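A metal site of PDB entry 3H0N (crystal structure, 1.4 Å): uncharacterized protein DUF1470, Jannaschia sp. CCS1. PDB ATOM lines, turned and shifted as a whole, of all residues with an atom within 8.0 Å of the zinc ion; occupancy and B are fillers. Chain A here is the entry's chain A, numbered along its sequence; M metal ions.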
ATOM      1  N   ASN A  20      -6.855 -22.314  12.936  1.00  0.00           N
ATOM      2  CA  ASN A  20      -7.578 -21.393  13.811  1.00  0.00           C
ATOM      3  C   ASN A  20      -7.671 -20.002  13.213  1.00  0.00           C
ATOM      4  O   ASN A  20      -8.643 -19.286  13.454  1.00  0.00           O
ATOM      5  CB  ASN A  20      -6.985 -21.424  15.206  1.00  0.00           C
ATOM      6  CG  ASN A  20      -7.448 -22.648  15.987  1.00  0.00           C
ATOM      7  OD1 ASN A  20      -8.500 -23.205  15.701  1.00  0.00           O
ATOM      8  ND2 ASN A  20      -6.655 -23.067  16.965  1.00  0.00           N
ATOM      9  N   SER A  26     -16.547 -19.972  14.697  1.00  0.00           N
ATOM     10  CA  SER A  26     -16.580 -19.000  15.794  1.00  0.00           C
ATOM     11  C   SER A  26     -15.275 -19.111  16.584  1.00  0.00           C
ATOM     12  O   SER A  26     -14.634 -20.160  16.613  1.00  0.00           O
ATOM     13  CB  SER A  26     -17.808 -19.186  16.696  1.00  0.00           C
ATOM     14  OG  SER A  26     -17.847 -20.455  17.310  1.00  0.00           O
ATOM     15  N   ARG A  27     -14.924 -18.007  17.237  1.00  0.00           N
ATOM     16  CA  ARG A  27     -13.683 -17.897  17.989  1.00  0.00           C
ATOM     17  C   ARG A  27     -13.927 -17.098  19.261  1.00  0.00           C
ATOM     18  O   ARG A  27     -14.358 -15.957  19.220  1.00  0.00           O
ATOM     19  CB  ARG A  27     -12.617 -17.237  17.130  1.00  0.00           C
ATOM     20  CG  ARG A  27     -11.334 -16.959  17.896  1.00  0.00           C
ATOM     21  CD  ARG A  27     -10.316 -16.286  16.996  1.00  0.00           C
ATOM     22  NE  ARG A  27      -9.058 -15.947  17.680  1.00  0.00           N
ATOM     23  CZ  ARG A  27      -8.869 -14.891  18.454  1.00  0.00           C
ATOM     24  NH1 ARG A  27      -9.830 -14.009  18.710  1.00  0.00           N
ATOM     25  NH2 ARG A  27      -7.661 -14.704  18.993  1.00  0.00           N
ATOM     26  N   ARG A  28     -13.741 -17.746  20.415  1.00  0.00           N
ATOM     27  CA  ARG A  28     -13.799 -17.036  21.691  1.00  0.00           C
ATOM     28  C   ARG A  28     -15.105 -16.289  21.900  1.00  0.00           C
ATOM     29  O   ARG A  28     -15.110 -15.208  22.473  1.00  0.00           O
ATOM     30  CB  ARG A  28     -12.573 -16.128  21.805  1.00  0.00           C
ATOM     31  CG  ARG A  28     -11.250 -16.915  21.797  1.00  0.00           C
ATOM     32  CD  ARG A  28     -10.065 -16.011  21.941  1.00  0.00           C
ATOM     33  NE  ARG A  28      -8.827 -16.748  21.821  1.00  0.00           N
ATOM     34  CZ  ARG A  28      -7.623 -16.251  22.099  1.00  0.00           C
ATOM     35  NH1 ARG A  28      -7.516 -14.992  22.536  1.00  0.00           N
ATOM     36  NH2 ARG A  28      -6.548 -17.010  21.949  1.00  0.00           N
ATOM     37  N   GLY A  29     -16.209 -16.882  21.456  1.00  0.00           N
ATOM     38  CA  GLY A  29     -17.547 -16.383  21.704  1.00  0.00           C
ATOM     39  C   GLY A  29     -18.160 -15.544  20.602  1.00  0.00           C
ATOM     40  O   GLY A  29     -19.313 -15.138  20.723  1.00  0.00           O
ATOM     41  N   ILE A 147     -12.018 -29.893  20.011  1.00  0.00           N
ATOM     42  CA  ILE A 147     -12.741 -28.698  19.547  1.00  0.00           C
ATOM     43  C   ILE A 147     -13.249 -27.991  20.801  1.00  0.00           C
ATOM     44  O   ILE A 147     -13.795 -28.610  21.711  1.00  0.00           O
ATOM     45  CB  ILE A 147     -13.954 -29.049  18.664  1.00  0.00           C
ATOM     46  CG1 ILE A 147     -13.595 -30.034  17.558  1.00  0.00           C
ATOM     47  CG2 ILE A 147     -14.603 -27.747  18.006  1.00  0.00           C
ATOM     48  CD1 ILE A 147     -12.593 -29.540  16.655  1.00  0.00           C
ATOM     49  N   CYS A 148     -12.988 -26.695  20.917  1.00  0.00           N
ATOM     50  CA  CYS A 148     -13.287 -25.920  22.120  1.00  0.00           C
ATOM     51  C   CYS A 148     -14.715 -26.154  22.623  1.00  0.00           C
ATOM     52  O   CYS A 148     -15.689 -26.065  21.846  1.00  0.00           O
ATOM     53  CB  CYS A 148     -13.097 -24.450  21.880  1.00  0.00           C
ATOM     54  SG  CYS A 148     -13.076 -23.497  23.388  1.00  0.00           S
ATOM     55  N   ASN A 149     -14.838 -26.359  23.910  1.00  0.00           N
ATOM     56  CA  ASN A 149     -16.150 -26.554  24.542  1.00  0.00           C
ATOM     57  C   ASN A 149     -16.880 -25.270  24.855  1.00  0.00           C
ATOM     58  O   ASN A 149     -18.032 -25.302  25.312  1.00  0.00           O
ATOM     59  CB  ASN A 149     -16.023 -27.436  25.794  1.00  0.00           C
ATOM     60  CG  ASN A 149     -15.999 -28.919  25.475  1.00  0.00           C
ATOM     61  OD1 ASN A 149     -16.213 -29.366  24.309  1.00  0.00           O
ATOM     62  ND2 ASN A 149     -15.970 -29.716  26.553  1.00  0.00           N
ATOM     63  N   ALA A 150     -16.257 -24.113  24.668  1.00  0.00           N
ATOM     64  CA  ALA A 150     -16.915 -22.874  25.032  1.00  0.00           C
ATOM     65  C   ALA A 150     -18.036 -22.549  24.046  1.00  0.00           C
ATOM     66  O   ALA A 150     -18.010 -22.978  22.890  1.00  0.00           O
ATOM     67  CB  ALA A 150     -15.888 -21.701  25.106  1.00  0.00           C
ATOM     68  N   HIS A 151     -18.989 -21.764  24.506  1.00  0.00           N
ATOM     69  CA  HIS A 151     -20.070 -21.290  23.654  1.00  0.00           C
ATOM     70  C   HIS A 151     -19.539 -20.417  22.546  1.00  0.00           C
ATOM     71  O   HIS A 151     -18.707 -19.487  22.747  1.00  0.00           O
ATOM     72  CB  HIS A 151     -21.068 -20.519  24.524  1.00  0.00           C
ATOM     73  CG  HIS A 151     -22.190 -19.854  23.756  1.00  0.00           C
ATOM     74  ND1 HIS A 151     -23.230 -20.587  23.217  1.00  0.00           N
ATOM     75  CD2 HIS A 151     -22.460 -18.552  23.480  1.00  0.00           C
ATOM     76  CE1 HIS A 151     -24.085 -19.748  22.655  1.00  0.00           C
ATOM     77  NE2 HIS A 151     -23.647 -18.521  22.794  1.00  0.00           N
ATOM     78  N   ARG A 152     -20.018 -20.678  21.322  1.00  0.00           N
ATOM     79  CA  ARG A 152     -19.555 -19.962  20.148  1.00  0.00           C
ATOM     80  C   ARG A 152     -18.016 -19.895  20.072  1.00  0.00           C
ATOM     81  O   ARG A 152     -17.398 -18.838  19.838  1.00  0.00           O
ATOM     82  CB  ARG A 152     -20.209 -18.579  20.018  1.00  0.00           C
ATOM     83  CG  ARG A 152     -21.629 -18.659  19.645  1.00  0.00           C
ATOM     84  CD  ARG A 152     -22.231 -17.302  19.415  1.00  0.00           C
ATOM     85  NE  ARG A 152     -23.613 -17.453  19.035  1.00  0.00           N
ATOM     86  CZ  ARG A 152     -24.425 -16.471  18.688  1.00  0.00           C
ATOM     87  NH1 ARG A 152     -23.996 -15.222  18.666  1.00  0.00           N
ATOM     88  NH2 ARG A 152     -25.654 -16.767  18.323  1.00  0.00           N
ATOM     89  N   CYS A 153     -17.423 -21.064  20.265  1.00  0.00           N
ATOM     90  CA  CYS A 153     -16.027 -21.247  19.867  1.00  0.00           C
ATOM     91  C   CYS A 153     -15.856 -22.617  19.304  1.00  0.00           C
ATOM     92  O   CYS A 153     -16.103 -23.598  20.028  1.00  0.00           O
ATOM     93  CB  CYS A 153     -15.101 -21.061  21.035  1.00  0.00           C
ATOM     94  SG  CYS A 153     -13.351 -21.025  20.510  1.00  0.00           S
ATOM     95  N   ASP A 154     -15.462 -22.725  18.039  1.00  0.00           N
ATOM     96  CA  ASP A 154     -15.079 -24.034  17.475  1.00  0.00           C
ATOM     97  C   ASP A 154     -13.640 -24.105  17.033  1.00  0.00           C
ATOM     98  O   ASP A 154     -13.274 -24.907  16.152  1.00  0.00           O
ATOM     99  CB  ASP A 154     -16.052 -24.482  16.396  1.00  0.00           C
ATOM    100  CG  ASP A 154     -15.945 -23.682  15.128  1.00  0.00           C
ATOM    101  OD1 ASP A 154     -15.323 -22.628  15.074  1.00  0.00           O
ATOM    102  OD2 ASP A 154     -16.531 -24.159  14.142  1.00  0.00           O
ATOM    103  N   ARG A 155     -12.817 -23.334  17.690  1.00  0.00           N
ATOM    104  CA  ARG A 155     -11.387 -23.433  17.459  1.00  0.00           C
ATOM    105  C   ARG A 155     -10.872 -24.782  17.948  1.00  0.00           C
ATOM    106  O   ARG A 155     -11.399 -25.393  18.867  1.00  0.00           O
ATOM    107  CB  ARG A 155     -10.629 -22.299  18.133  1.00  0.00           C
ATOM    108  CG  ARG A 155     -11.011 -20.907  17.693  1.00  0.00           C
ATOM    109  CD  ARG A 155     -10.877 -20.651  16.214  1.00  0.00           C
ATOM    110  NE  ARG A 155     -12.064 -21.009  15.481  1.00  0.00           N
ATOM    111  CZ  ARG A 155     -12.157 -20.996  14.140  1.00  0.00           C
ATOM    112  NH1 ARG A 155     -11.150 -20.624  13.370  1.00  0.00           N
ATOM    113  NH2 ARG A 155     -13.295 -21.340  13.537  1.00  0.00           N
ATOM    114  N   VAL A 156      -9.808 -25.220  17.297  1.00  0.00           N
ATOM    115  CA  VAL A 156      -9.183 -26.523  17.585  1.00  0.00           C
ATOM    116  C   VAL A 156      -8.014 -26.336  18.553  1.00  0.00           C
ATOM    117  O   VAL A 156      -7.428 -25.268  18.699  1.00  0.00           O
ATOM    118  CB  VAL A 156      -8.703 -27.242  16.310  1.00  0.00           C
ATOM    119  CG1 VAL A 156      -9.870 -27.492  15.354  1.00  0.00           C
ATOM    120  CG2 VAL A 156      -7.550 -26.552  15.621  1.00  0.00           C
ATOM    121  N   TYR A 157      -7.684 -27.450  19.223  1.00  0.00           N
ATOM    122  CA  TYR A 157      -6.531 -27.444  20.118  1.00  0.00           C
ATOM    123  C   TYR A 157      -5.971 -28.833  20.229  1.00  0.00           C
ATOM    124  O   TYR A 157      -6.629 -29.828  19.910  1.00  0.00           O
ATOM    125  CB  TYR A 157      -6.898 -26.849  21.497  1.00  0.00           C
ATOM    126  CG  TYR A 157      -7.870 -27.669  22.292  1.00  0.00           C
ATOM    127  CD1 TYR A 157      -9.257 -27.527  22.062  1.00  0.00           C
ATOM    128  CD2 TYR A 157      -7.475 -28.586  23.256  1.00  0.00           C
ATOM    129  CE1 TYR A 157     -10.160 -28.280  22.775  1.00  0.00           C
ATOM    130  CE2 TYR A 157      -8.379 -29.307  23.978  1.00  0.00           C
ATOM    131  CZ  TYR A 157      -9.732 -29.197  23.698  1.00  0.00           C
ATOM    132  OH  TYR A 157     -10.652 -29.936  24.401  1.00  0.00           O
ATOM    133  N   GLN A 167     -10.394 -28.932  28.029  1.00  0.00           N
ATOM    134  CA  GLN A 167     -11.714 -28.779  27.398  1.00  0.00           C
ATOM    135  C   GLN A 167     -11.791 -27.577  26.466  1.00  0.00           C
ATOM    136  O   GLN A 167     -12.695 -27.505  25.649  1.00  0.00           O
ATOM    137  CB  GLN A 167     -12.813 -28.629  28.490  1.00  0.00           C
ATOM    138  CG  GLN A 167     -12.946 -29.871  29.372  1.00  0.00           C
ATOM    139  CD  GLN A 167     -13.958 -29.749  30.525  1.00  0.00           C
ATOM    140  OE1 GLN A 167     -14.232 -28.667  31.047  1.00  0.00           O
ATOM    141  NE2 GLN A 167     -14.532 -30.891  30.902  1.00  0.00           N
ATOM    142  N   TYR A 168     -10.901 -26.603  26.646  1.00  0.00           N
ATOM    143  CA  TYR A 168     -10.983 -25.295  26.020  1.00  0.00           C
ATOM    144  C   TYR A 168      -9.736 -24.991  25.244  1.00  0.00           C
ATOM    145  O   TYR A 168      -8.628 -25.406  25.633  1.00  0.00           O
ATOM    146  CB  TYR A 168     -11.289 -24.174  27.061  1.00  0.00           C
ATOM    147  CG  TYR A 168     -12.575 -24.461  27.856  1.00  0.00           C
ATOM    148  CD1 TYR A 168     -13.811 -24.414  27.239  1.00  0.00           C
ATOM    149  CD2 TYR A 168     -12.550 -24.855  29.171  1.00  0.00           C
ATOM    150  CE1 TYR A 168     -14.950 -24.723  27.936  1.00  0.00           C
ATOM    151  CE2 TYR A 168     -13.704 -25.180  29.858  1.00  0.00           C
ATOM    152  CZ  TYR A 168     -14.884 -25.111  29.240  1.00  0.00           C
ATOM    153  OH  TYR A 168     -16.073 -25.431  29.877  1.00  0.00           O
ATOM    154  N   CYS A 169      -9.897 -24.212  24.186  1.00  0.00           N
ATOM    155  CA  CYS A 169      -8.824 -23.960  23.221  1.00  0.00           C
ATOM    156  C   CYS A 169      -7.755 -23.024  23.713  1.00  0.00           C
ATOM    157  O   CYS A 169      -6.704 -22.929  23.104  1.00  0.00           O
ATOM    158  CB  CYS A 169      -9.361 -23.379  21.908  1.00  0.00           C
ATOM    159  SG  CYS A 169      -9.987 -21.673  22.057  1.00  0.00           S
ATOM    160  N   SER A 170      -8.045 -22.304  24.798  1.00  0.00           N
ATOM    161  CA  SER A 170      -7.256 -21.147  25.191  1.00  0.00           C
ATOM    162  C   SER A 170      -7.550 -20.739  26.587  1.00  0.00           C
ATOM    163  O   SER A 170      -8.602 -21.029  27.143  1.00  0.00           O
ATOM    164  CB  SER A 170      -7.547 -19.972  24.299  1.00  0.00           C
ATOM    165  OG  SER A 170      -8.874 -19.561  24.359  1.00  0.00           O
ATOM    166  N   LEU A 171      -6.612 -19.991  27.145  1.00  0.00           N
ATOM    167  CA  LEU A 171      -6.845 -19.358  28.433  1.00  0.00           C
ATOM    168  C   LEU A 171      -8.023 -18.391  28.335  1.00  0.00           C
ATOM    169  O   LEU A 171      -8.826 -18.261  29.258  1.00  0.00           O
ATOM    170  CB  LEU A 171      -5.558 -18.682  28.915  1.00  0.00           C
ATOM    171  CG  LEU A 171      -5.626 -17.974  30.241  1.00  0.00           C
ATOM    172  CD1 LEU A 171      -6.057 -18.884  31.351  1.00  0.00           C
ATOM    173  CD2 LEU A 171      -4.236 -17.318  30.534  1.00  0.00           C
ATOM    174  N   ALA A 172      -8.206 -17.752  27.181  1.00  0.00           N
ATOM    175  CA  ALA A 172      -9.278 -16.844  26.975  1.00  0.00           C
ATOM    176  C   ALA A 172     -10.629 -17.530  27.214  1.00  0.00           C
ATOM    177  O   ALA A 172     -11.476 -17.069  27.975  1.00  0.00           O
ATOM    178  CB  ALA A 172      -9.190 -16.217  25.563  1.00  0.00           C
ATOM    179  N   CYS A 173     -10.842 -18.687  26.583  1.00  0.00           N
ATOM    180  CA  CYS A 173     -12.084 -19.408  26.753  1.00  0.00           C
ATOM    181  C   CYS A 173     -12.197 -20.024  28.144  1.00  0.00           C
ATOM    182  O   CYS A 173     -13.275 -20.023  28.721  1.00  0.00           O
ATOM    183  CB  CYS A 173     -12.231 -20.470  25.658  1.00  0.00           C
ATOM    184  SG  CYS A 173     -12.520 -19.762  23.992  1.00  0.00           S
ATOM    185  N   GLN A 174     -11.108 -20.527  28.686  1.00  0.00           N
ATOM    186  CA  GLN A 174     -11.080 -20.981  30.073  1.00  0.00           C
ATOM    187  C   GLN A 174     -11.591 -19.857  31.013  1.00  0.00           C
ATOM    188  O   GLN A 174     -12.363 -20.112  31.929  1.00  0.00           O
ATOM    189  CB  GLN A 174      -9.659 -21.458  30.445  1.00  0.00           C
ATOM    190  CG  GLN A 174      -9.566 -22.278  31.695  1.00  0.00           C
ATOM    191  CD  GLN A 174      -9.885 -23.762  31.445  1.00  0.00           C
ATOM    192  OE1 GLN A 174      -9.342 -24.412  30.519  1.00  0.00           O
ATOM    193  NE2 GLN A 174     -10.686 -24.330  32.332  1.00  0.00           N
ATOM    194  N   ARG A 176     -13.346 -17.057  30.229  1.00  0.00           N
ATOM    195  CA  ARG A 176     -14.741 -16.673  29.940  1.00  0.00           C
ATOM    196  C   ARG A 176     -15.728 -17.599  30.628  1.00  0.00           C
ATOM    197  O   ARG A 176     -16.684 -17.164  31.240  1.00  0.00           O
ATOM    198  CB  ARG A 176     -14.966 -16.653  28.447  1.00  0.00           C
ATOM    199  CG  ARG A 176     -16.300 -16.015  28.030  1.00  0.00           C
ATOM    200  CD  ARG A 176     -16.409 -15.908  26.525  1.00  0.00           C
ATOM    201  NE  ARG A 176     -15.069 -15.838  25.977  1.00  0.00           N
ATOM    202  CZ  ARG A 176     -14.446 -16.801  25.303  1.00  0.00           C
ATOM    203  NH1 ARG A 176     -15.055 -17.951  24.970  1.00  0.00           N
ATOM    204  NH2 ARG A 176     -13.188 -16.597  24.920  1.00  0.00           N
ATOM    205  N   VAL A 177     -15.445 -18.885  30.594  1.00  0.00           N
ATOM    206  CA  VAL A 177     -16.251 -19.891  31.286  1.00  0.00           C
ATOM    207  C   VAL A 177     -16.234 -19.702  32.780  1.00  0.00           C
ATOM    208  O   VAL A 177     -17.264 -19.713  33.407  1.00  0.00           O
ATOM    209  CB  VAL A 177     -15.780 -21.311  30.886  1.00  0.00           C
ATOM    210  CG1 VAL A 177     -16.439 -22.360  31.781  1.00  0.00           C
ATOM    211  CG2 VAL A 177     -16.114 -21.538  29.362  1.00  0.00           C
HETATM  212 ZN    ZN M   1     -12.266 -21.508  22.522  1.00  0.00          ZN
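SG of Cys 153 lies close to N of Arg 28.
The backbone NH (N) of Cys 173 sits at hydrogen-bond distance from the side-chain hydroxyl (OG) of Ser 170, at 3.1 Å.
N of Arg 155 lies close to SG of Cys 153 (3.7 Å).
SG of Cys 148 lies close to N of Ala 150, at 3.5 Å.
N of Cys 148 sits at hydrogen-bond distance from O of Arg 155, 2.9 Å away.
The guanidinium group of Arg 176 sits close to the side-chain sulfur of Cys 173.
The side-chain sulfur (SG) of Cys 169 lies close to the side-chain hydroxyl (OG) of Ser 170, 3.3 Å away.
N of Cys 153 sits at hydrogen-bond distance from OG of Ser 26, at 3.0 Å.
Within 4 Å of the zinc ion: Cys 148, Cys 153, Cys 169 and Cys 173.
The nearest printed residue that does not touch the zinc ion is Ser 170 (4.3 Å).
The zinc ion is bound by SG of Cys 173, at 2.3 Å.
The zinc ion is bound by SG of Cys 148, at 2.3 Å.
The zinc ion is bound by the side-chain sulfur (SG) of Cys 169 (2.3 Å).
SG of Cys 153 is bound to the zinc ion (2.3 Å).
The zinc ion has four donor atoms within binding distance.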
